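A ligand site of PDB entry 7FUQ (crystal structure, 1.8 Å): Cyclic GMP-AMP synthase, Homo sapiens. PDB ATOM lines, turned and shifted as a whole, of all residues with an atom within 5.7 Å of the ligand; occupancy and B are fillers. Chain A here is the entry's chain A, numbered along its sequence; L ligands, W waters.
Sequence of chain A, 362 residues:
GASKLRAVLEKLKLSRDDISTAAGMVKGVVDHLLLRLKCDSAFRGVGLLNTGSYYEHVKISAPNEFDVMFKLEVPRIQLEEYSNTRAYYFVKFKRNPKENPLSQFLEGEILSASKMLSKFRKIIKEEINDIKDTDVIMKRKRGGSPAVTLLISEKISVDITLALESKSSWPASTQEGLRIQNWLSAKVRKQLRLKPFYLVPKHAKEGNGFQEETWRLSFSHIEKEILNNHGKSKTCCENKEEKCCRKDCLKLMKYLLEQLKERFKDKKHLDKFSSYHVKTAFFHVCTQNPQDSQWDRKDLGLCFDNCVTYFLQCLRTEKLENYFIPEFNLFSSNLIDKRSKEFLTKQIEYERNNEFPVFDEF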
ATOM      1  N   LYS A  59     -30.175  -0.368  12.166  1.00  0.00           N
ATOM      2  CA  LYS A  59     -29.038  -0.419  13.080  1.00  0.00           C
ATOM      3  C   LYS A  59     -27.756  -0.221  12.271  1.00  0.00           C
ATOM      4  O   LYS A  59     -27.640  -0.731  11.152  1.00  0.00           O
ATOM      5  CB  LYS A  59     -29.009  -1.785  13.793  1.00  0.00           C
ATOM      6  CG  LYS A  59     -28.751  -1.764  15.301  1.00  0.00           C
ATOM      7  CD  LYS A  59     -29.019  -3.141  15.956  1.00  0.00           C
ATOM      8  CE  LYS A  59     -29.047  -3.010  17.507  1.00  0.00           C
ATOM      9  NZ  LYS A  59     -29.070  -4.298  18.341  1.00  0.00           N
ATOM     10  N   SER A 145     -27.541 -16.693   8.711  1.00  0.00           N
ATOM     11  CA  SER A 145     -28.052 -15.415   9.146  1.00  0.00           C
ATOM     12  C   SER A 145     -26.922 -14.399   9.157  1.00  0.00           C
ATOM     13  O   SER A 145     -25.856 -14.679   9.729  1.00  0.00           O
ATOM     14  CB  SER A 145     -28.683 -15.519  10.551  1.00  0.00           C
ATOM     15  OG  SER A 145     -28.596 -14.280  11.230  1.00  0.00           O
ATOM     16  N   LEU A 178     -28.986 -11.291  31.405  1.00  0.00           N
ATOM     17  CA  LEU A 178     -29.472  -9.911  31.561  1.00  0.00           C
ATOM     18  C   LEU A 178     -29.291  -9.456  33.012  1.00  0.00           C
ATOM     19  O   LEU A 178     -30.239  -9.106  33.711  1.00  0.00           O
ATOM     20  CB  LEU A 178     -30.933  -9.801  31.117  1.00  0.00           C
ATOM     21  CG  LEU A 178     -31.501  -8.373  30.952  1.00  0.00           C
ATOM     22  CD1 LEU A 178     -30.796  -7.544  29.917  1.00  0.00           C
ATOM     23  CD2 LEU A 178     -32.993  -8.433  30.643  1.00  0.00           C
ATOM     24  N   VAL A 200     -33.830 -16.399  15.203  1.00  0.00           N
ATOM     25  CA  VAL A 200     -33.324 -16.171  13.849  1.00  0.00           C
ATOM     26  C   VAL A 200     -32.674 -17.447  13.318  1.00  0.00           C
ATOM     27  O   VAL A 200     -32.120 -18.233  14.104  1.00  0.00           O
ATOM     28  CB  VAL A 200     -32.347 -14.995  13.794  1.00  0.00           C
ATOM     29  CG1 VAL A 200     -32.980 -13.762  14.408  1.00  0.00           C
ATOM     30  CG2 VAL A 200     -31.060 -15.330  14.512  1.00  0.00           C
ATOM     31  N   LYS A 202     -29.953 -18.522  12.361  1.00  0.00           N
ATOM     32  CA  LYS A 202     -28.506 -18.739  12.422  1.00  0.00           C
ATOM     33  C   LYS A 202     -28.279 -20.192  12.815  1.00  0.00           C
ATOM     34  O   LYS A 202     -28.613 -20.598  13.933  1.00  0.00           O
ATOM     35  CB  LYS A 202     -27.856 -17.777  13.415  1.00  0.00           C
ATOM     36  CG  LYS A 202     -26.348 -17.955  13.528  1.00  0.00           C
ATOM     37  CD  LYS A 202     -25.692 -16.681  14.031  1.00  0.00           C
ATOM     38  CE  LYS A 202     -24.169 -16.828  14.120  1.00  0.00           C
ATOM     39  NZ  LYS A 202     -23.759 -17.687  15.270  1.00  0.00           N
ATOM     40  N   ARG A 216     -31.629 -19.542  16.403  1.00  0.00           N
ATOM     41  CA  ARG A 216     -30.894 -18.953  17.516  1.00  0.00           C
ATOM     42  C   ARG A 216     -31.753 -17.915  18.235  1.00  0.00           C
ATOM     43  O   ARG A 216     -32.429 -17.111  17.577  1.00  0.00           O
ATOM     44  CB  ARG A 216     -29.595 -18.317  17.021  1.00  0.00           C
ATOM     45  CG  ARG A 216     -28.858 -17.510  18.101  1.00  0.00           C
ATOM     46  CD  ARG A 216     -27.455 -17.188  17.709  1.00  0.00           C
ATOM     47  NE  ARG A 216     -26.859 -16.216  18.619  1.00  0.00           N
ATOM     48  CZ  ARG A 216     -25.556 -15.967  18.712  1.00  0.00           C
ATOM     49  NH1 ARG A 216     -24.701 -16.648  17.963  1.00  0.00           N
ATOM     50  NH2 ARG A 216     -25.124 -15.040  19.556  1.00  0.00           N
ATOM     51  N   LEU A 217     -31.754 -17.943  19.568  1.00  0.00           N
ATOM     52  CA  LEU A 217     -32.408 -16.906  20.357  1.00  0.00           C
ATOM     53  C   LEU A 217     -31.794 -15.548  20.052  1.00  0.00           C
ATOM     54  O   LEU A 217     -30.570 -15.419  19.950  1.00  0.00           O
ATOM     55  CB  LEU A 217     -32.261 -17.173  21.856  1.00  0.00           C
ATOM     56  CG  LEU A 217     -32.920 -18.382  22.477  1.00  0.00           C
ATOM     57  CD1 LEU A 217     -32.719 -18.352  23.975  1.00  0.00           C
ATOM     58  CD2 LEU A 217     -34.391 -18.354  22.143  1.00  0.00           C
ATOM     59  N   SER A 218     -32.634 -14.538  19.926  1.00  0.00           N
ATOM     60  CA  SER A 218     -32.142 -13.202  19.626  1.00  0.00           C
ATOM     61  C   SER A 218     -32.805 -12.182  20.526  1.00  0.00           C
ATOM     62  O   SER A 218     -34.033 -12.166  20.674  1.00  0.00           O
ATOM     63  CB  SER A 218     -32.377 -12.834  18.169  1.00  0.00           C
ATOM     64  OG  SER A 218     -31.846 -11.554  17.918  1.00  0.00           O
ATOM     65  N   PHE A 219     -31.985 -11.315  21.117  1.00  0.00           N
ATOM     66  CA  PHE A 219     -32.495 -10.252  21.976  1.00  0.00           C
ATOM     67  C   PHE A 219     -31.972  -8.901  21.525  1.00  0.00           C
ATOM     68  O   PHE A 219     -31.890  -7.965  22.324  1.00  0.00           O
ATOM     69  CB  PHE A 219     -32.125 -10.535  23.433  1.00  0.00           C
ATOM     70  CG  PHE A 219     -32.676 -11.829  23.942  1.00  0.00           C
ATOM     71  CD1 PHE A 219     -33.955 -11.884  24.499  1.00  0.00           C
ATOM     72  CD2 PHE A 219     -31.937 -13.001  23.864  1.00  0.00           C
ATOM     73  CE1 PHE A 219     -34.477 -13.092  24.959  1.00  0.00           C
ATOM     74  CE2 PHE A 219     -32.458 -14.197  24.331  1.00  0.00           C
ATOM     75  CZ  PHE A 219     -33.723 -14.238  24.878  1.00  0.00           C
ATOM     76  N   SER A 220     -31.632  -8.771  20.235  1.00  0.00           N
ATOM     77  CA  SER A 220     -31.044  -7.540  19.731  1.00  0.00           C
ATOM     78  C   SER A 220     -31.955  -6.342  19.957  1.00  0.00           C
ATOM     79  O   SER A 220     -31.470  -5.219  20.104  1.00  0.00           O
ATOM     80  CB  SER A 220     -30.722  -7.688  18.246  1.00  0.00           C
ATOM     81  OG  SER A 220     -30.448  -6.416  17.682  1.00  0.00           O
ATOM     82  N   HIS A 221     -33.269  -6.559  19.990  1.00  0.00           N
ATOM     83  CA  HIS A 221     -34.246  -5.489  20.185  1.00  0.00           C
ATOM     84  C   HIS A 221     -34.190  -4.891  21.586  1.00  0.00           C
ATOM     85  O   HIS A 221     -34.829  -3.851  21.821  1.00  0.00           O
ATOM     86  CB  HIS A 221     -35.657  -6.016  19.917  1.00  0.00           C
ATOM     87  CG  HIS A 221     -36.069  -7.100  20.876  1.00  0.00           C
ATOM     88  ND1 HIS A 221     -35.344  -8.252  21.040  1.00  0.00           N
ATOM     89  CD2 HIS A 221     -37.115  -7.177  21.729  1.00  0.00           C
ATOM     90  CE1 HIS A 221     -35.942  -9.018  21.937  1.00  0.00           C
ATOM     91  NE2 HIS A 221     -37.027  -8.388  22.373  1.00  0.00           N
ATOM     92  N   ILE A 222     -33.508  -5.536  22.527  1.00  0.00           N
ATOM     93  CA  ILE A 222     -33.422  -4.966  23.863  1.00  0.00           C
ATOM     94  C   ILE A 222     -32.363  -3.877  23.934  1.00  0.00           C
ATOM     95  O   ILE A 222     -32.399  -3.049  24.852  1.00  0.00           O
ATOM     96  CB  ILE A 222     -33.157  -6.080  24.897  1.00  0.00           C
ATOM     97  CG1 ILE A 222     -34.266  -7.150  24.852  1.00  0.00           C
ATOM     98  CG2 ILE A 222     -32.900  -5.519  26.333  1.00  0.00           C
ATOM     99  CD1 ILE A 222     -35.655  -6.684  25.237  1.00  0.00           C
ATOM    100  N   GLU A 223     -31.448  -3.807  22.965  1.00  0.00           N
ATOM    101  CA  GLU A 223     -30.341  -2.871  23.082  1.00  0.00           C
ATOM    102  C   GLU A 223     -30.853  -1.439  23.193  1.00  0.00           C
ATOM    103  O   GLU A 223     -30.439  -0.695  24.097  1.00  0.00           O
ATOM    104  CB  GLU A 223     -29.371  -2.979  21.910  1.00  0.00           C
ATOM    105  CG  GLU A 223     -28.122  -2.131  22.204  1.00  0.00           C
ATOM    106  CD  GLU A 223     -27.143  -2.008  21.033  1.00  0.00           C
ATOM    107  OE1 GLU A 223     -27.389  -2.592  19.964  1.00  0.00           O
ATOM    108  OE2 GLU A 223     -26.107  -1.326  21.205  1.00  0.00           O
ATOM    109  N   ILE A 226     -32.052  -0.136  26.533  1.00  0.00           N
ATOM    110  CA  ILE A 226     -31.078   0.069  27.595  1.00  0.00           C
ATOM    111  C   ILE A 226     -30.067   1.152  27.228  1.00  0.00           C
ATOM    112  O   ILE A 226     -29.695   1.963  28.077  1.00  0.00           O
ATOM    113  CB  ILE A 226     -30.386  -1.265  27.938  1.00  0.00           C
ATOM    114  CG1 ILE A 226     -31.355  -2.137  28.748  1.00  0.00           C
ATOM    115  CG2 ILE A 226     -29.084  -1.023  28.725  1.00  0.00           C
ATOM    116  CD1 ILE A 226     -30.900  -3.531  28.932  1.00  0.00           C
ATOM    117  N   TYR A 276     -20.865  -6.506  17.548  1.00  0.00           N
ATOM    118  CA  TYR A 276     -21.620  -7.300  18.529  1.00  0.00           C
ATOM    119  C   TYR A 276     -20.739  -7.759  19.697  1.00  0.00           C
ATOM    120  O   TYR A 276     -21.183  -7.749  20.845  1.00  0.00           O
ATOM    121  CB  TYR A 276     -22.268  -8.489  17.830  1.00  0.00           C
ATOM    122  CG  TYR A 276     -22.973  -9.490  18.739  1.00  0.00           C
ATOM    123  CD1 TYR A 276     -23.909  -9.090  19.698  1.00  0.00           C
ATOM    124  CD2 TYR A 276     -22.727 -10.862  18.600  1.00  0.00           C
ATOM    125  CE1 TYR A 276     -24.561 -10.025  20.495  1.00  0.00           C
ATOM    126  CE2 TYR A 276     -23.365 -11.796  19.380  1.00  0.00           C
ATOM    127  CZ  TYR A 276     -24.277 -11.384  20.319  1.00  0.00           C
ATOM    128  OH  TYR A 276     -24.890 -12.355  21.063  1.00  0.00           O
ATOM    129  N   LYS A 279     -20.058  -4.577  21.829  1.00  0.00           N
ATOM    130  CA  LYS A 279     -21.235  -4.196  22.602  1.00  0.00           C
ATOM    131  C   LYS A 279     -21.427  -5.117  23.797  1.00  0.00           C
ATOM    132  O   LYS A 279     -21.752  -4.656  24.889  1.00  0.00           O
ATOM    133  CB  LYS A 279     -22.503  -4.252  21.751  1.00  0.00           C
ATOM    134  CG  LYS A 279     -22.689  -3.225  20.691  1.00  0.00           C
ATOM    135  CD  LYS A 279     -23.961  -3.580  19.939  1.00  0.00           C
ATOM    136  CE  LYS A 279     -24.133  -2.722  18.736  1.00  0.00           C
ATOM    137  NZ  LYS A 279     -25.521  -2.822  18.266  1.00  0.00           N
ATOM    138  N   THR A 280     -21.300  -6.439  23.569  1.00  0.00           N
ATOM    139  CA  THR A 280     -21.489  -7.401  24.655  1.00  0.00           C
ATOM    140  C   THR A 280     -20.489  -7.135  25.777  1.00  0.00           C
ATOM    141  O   THR A 280     -20.867  -7.063  26.955  1.00  0.00           O
ATOM    142  CB  THR A 280     -21.331  -8.834  24.114  1.00  0.00           C
ATOM    143  OG1 THR A 280     -22.329  -9.083  23.115  1.00  0.00           O
ATOM    144  CG2 THR A 280     -21.464  -9.862  25.237  1.00  0.00           C
ATOM    145  N   PHE A 283     -21.520  -3.913  27.695  1.00  0.00           N
ATOM    146  CA  PHE A 283     -22.624  -4.032  28.646  1.00  0.00           C
ATOM    147  C   PHE A 283     -22.255  -4.884  29.856  1.00  0.00           C
ATOM    148  O   PHE A 283     -22.772  -4.650  30.952  1.00  0.00           O
ATOM    149  CB  PHE A 283     -23.892  -4.564  27.941  1.00  0.00           C
ATOM    150  CG  PHE A 283     -24.552  -3.510  27.088  1.00  0.00           C
ATOM    151  CD1 PHE A 283     -25.099  -2.359  27.681  1.00  0.00           C
ATOM    152  CD2 PHE A 283     -24.607  -3.637  25.701  1.00  0.00           C
ATOM    153  CE1 PHE A 283     -25.686  -1.363  26.891  1.00  0.00           C
ATOM    154  CE2 PHE A 283     -25.207  -2.626  24.913  1.00  0.00           C
ATOM    155  CZ  PHE A 283     -25.742  -1.495  25.525  1.00  0.00           C
ATOM    156  N   ASN A 322     -22.460 -14.471  26.146  1.00  0.00           N
ATOM    157  CA  ASN A 322     -23.670 -13.849  25.632  1.00  0.00           C
ATOM    158  C   ASN A 322     -24.379 -13.111  26.770  1.00  0.00           C
ATOM    159  O   ASN A 322     -24.556 -13.659  27.866  1.00  0.00           O
ATOM    160  CB  ASN A 322     -24.559 -14.943  25.038  1.00  0.00           C
ATOM    161  CG  ASN A 322     -25.830 -14.419  24.363  1.00  0.00           C
ATOM    162  OD1 ASN A 322     -26.643 -13.743  24.979  1.00  0.00           O
ATOM    163  ND2 ASN A 322     -26.013 -14.778  23.081  1.00  0.00           N
ATOM    164  N   TYR A 323     -24.760 -11.852  26.517  1.00  0.00           N
ATOM    165  CA  TYR A 323     -25.340 -11.031  27.576  1.00  0.00           C
ATOM    166  C   TYR A 323     -26.617 -11.623  28.132  1.00  0.00           C
ATOM    167  O   TYR A 323     -26.974 -11.360  29.294  1.00  0.00           O
ATOM    168  CB  TYR A 323     -25.601  -9.610  27.074  1.00  0.00           C
ATOM    169  CG  TYR A 323     -25.671  -8.592  28.212  1.00  0.00           C
ATOM    170  CD1 TYR A 323     -24.534  -8.310  28.972  1.00  0.00           C
ATOM    171  CD2 TYR A 323     -26.866  -7.939  28.536  1.00  0.00           C
ATOM    172  CE1 TYR A 323     -24.586  -7.419  30.031  1.00  0.00           C
ATOM    173  CE2 TYR A 323     -26.917  -7.019  29.589  1.00  0.00           C
ATOM    174  CZ  TYR A 323     -25.767  -6.764  30.338  1.00  0.00           C
ATOM    175  OH  TYR A 323     -25.801  -5.855  31.379  1.00  0.00           O
ATOM    176  N   PHE A 324     -27.336 -12.417  27.331  1.00  0.00           N
ATOM    177  CA  PHE A 324     -28.615 -12.978  27.729  1.00  0.00           C
ATOM    178  C   PHE A 324     -28.541 -14.462  28.032  1.00  0.00           C
ATOM    179  O   PHE A 324     -29.422 -14.963  28.726  1.00  0.00           O
ATOM    180  CB  PHE A 324     -29.659 -12.757  26.608  1.00  0.00           C
ATOM    181  CG  PHE A 324     -29.968 -11.317  26.407  1.00  0.00           C
ATOM    182  CD1 PHE A 324     -29.082 -10.513  25.730  1.00  0.00           C
ATOM    183  CD2 PHE A 324     -31.102 -10.753  26.970  1.00  0.00           C
ATOM    184  CE1 PHE A 324     -29.324  -9.172  25.578  1.00  0.00           C
ATOM    185  CE2 PHE A 324     -31.347  -9.392  26.840  1.00  0.00           C
ATOM    186  CZ  PHE A 324     -30.467  -8.600  26.128  1.00  0.00           C
HETATM  187  C1  LIG L   1     -26.703  -8.541  17.426  1.00  0.00           C
HETATM  188  C2  LIG L   1     -27.412 -10.934  17.505  1.00  0.00           C
HETATM  189  C3  LIG L   1     -28.891 -12.623  16.649  1.00  0.00           C
HETATM  190  C4  LIG L   1     -27.806 -13.448  16.398  1.00  0.00           C
HETATM  191  C5  LIG L   1     -26.528 -13.012  16.701  1.00  0.00           C
HETATM  192  C6  LIG L   1     -26.318 -11.766  17.266  1.00  0.00           C
HETATM  193  C7  LIG L   1     -27.834  -6.930  23.014  1.00  0.00           C
HETATM  194  C8  LIG L   1     -26.711  -6.766  23.847  1.00  0.00           C
HETATM  195  C9  LIG L   1     -26.797  -6.087  25.042  1.00  0.00           C
HETATM  196  C10 LIG L   1     -27.999  -5.541  25.474  1.00  0.00           C
HETATM  197  C11 LIG L   1     -29.117  -5.705  24.669  1.00  0.00           C
HETATM  198  C12 LIG L   1     -29.048  -6.397  23.471  1.00  0.00           C
HETATM  199  C13 LIG L   1     -28.070  -4.778  26.775  1.00  0.00           C
HETATM  200  C14 LIG L   1     -28.091  -9.045  21.730  1.00  0.00           C
HETATM  201  C15 LIG L   1     -28.700 -11.367  17.211  1.00  0.00           C
HETATM  202  C16 LIG L   1     -27.745  -7.696  21.745  1.00  0.00           C
HETATM  203  C17 LIG L   1     -27.221  -7.112  20.595  1.00  0.00           C
HETATM  204  C18 LIG L   1     -27.095  -7.854  19.419  1.00  0.00           C
HETATM  205  C19 LIG L   1     -27.478  -9.206  19.398  1.00  0.00           C
HETATM  206  C20 LIG L   1     -27.986  -9.805  20.559  1.00  0.00           C
HETATM  207  C21 LIG L   1     -28.384 -11.249  20.677  1.00  0.00           C
HETATM  208  N1  LIG L   1     -27.213  -9.632  18.073  1.00  0.00           N
HETATM  209  N2  LIG L   1     -26.616  -7.472  18.167  1.00  0.00           N
HETATM  210  O1  LIG L   1     -29.439 -11.503  21.385  1.00  0.00           O
HETATM  211  O2  LIG L   1     -27.712 -12.147  20.190  1.00  0.00           O
HETATM  212 CL1  LIG L   1     -25.169  -7.417  23.374  1.00  0.00          CL
HETATM  213  O   HOH W   1     -28.528 -14.390  21.657  1.00  0.00           O
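The backbone NH (N) of Phe 219 lies within hydrogen-bond range of an oxygen (O1) of the ligand, 2.6 Å away.
O2 of the ligand sits at hydrogen-bond distance from OH of Tyr 276, 3.0 Å away.
NH2 of Arg 216 is in salt-bridge range of O2 of the ligand.
Merely in contact with the ligand: Ser 218 (3.2 Å), Ser 220 (3.7 Å), Ile 222 (3.8 Å), Glu 223 (3.5 Å), Ile 226 (3.8 Å), Thr 280 (3.3 Å), Phe 283 (3.4 Å), Tyr 323 (3.8 Å) and Phe 324 (3.5 Å).
Hydrophobic or aromatic side chains that line the ligand: Phe 219, Ile 226, Tyr 276, Phe 283, Tyr 323 and Phe 324.
12 residues have an atom within 4 Å of the ligand: Arg 216, Ser 218, Phe 219, Ser 220, Ile 222, Glu 223, Ile 226, Tyr 276, Thr 280, Phe 283, Tyr 323 and Phe 324.
The nearest printed residue that does not touch the ligand is Lys 59 (4.02 Å).
O of Tyr 276 sits at hydrogen-bond distance from OG1 of Thr 280.
The side-chain hydroxyl of Tyr 276 sits at hydrogen-bond distance from the guanidinium group of Arg 216 (3.1 Å).
The side-chain hydroxyl of Tyr 276 lies within hydrogen-bond range of the side-chain amide nitrogen of Asn 322, at 3.3 Å.
The backbone carbonyl oxygen (O) of Phe 283 is in hydrogen-bond range of the side-chain hydroxyl (OH) of Tyr 323 (3.3 Å).
The side-chain carboxylate (OE1) of Glu 223 lies within salt-bridge range of the side-chain amino group (NZ) of Lys 279 (2.5 Å).
The side-chain amide oxygen of Asn 322 lies within hydrogen-bond range of the backbone NH of Phe 324, at 2.8 Å.
The backbone NH (N) of Arg 216 is in hydrogen-bond range of the backbone carbonyl oxygen (O) of Val 200 (2.7 Å).
The side-chain hydroxyl of Ser 220 is in hydrogen-bond range of the side-chain amino group of Lys 59 (2.6 Å).
Water W1 lies within hydrogen-bond range of an oxygen (O2) of the ligand, the backbone carbonyl oxygen of Leu 217 and the side-chain amide nitrogen of Asn 322.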
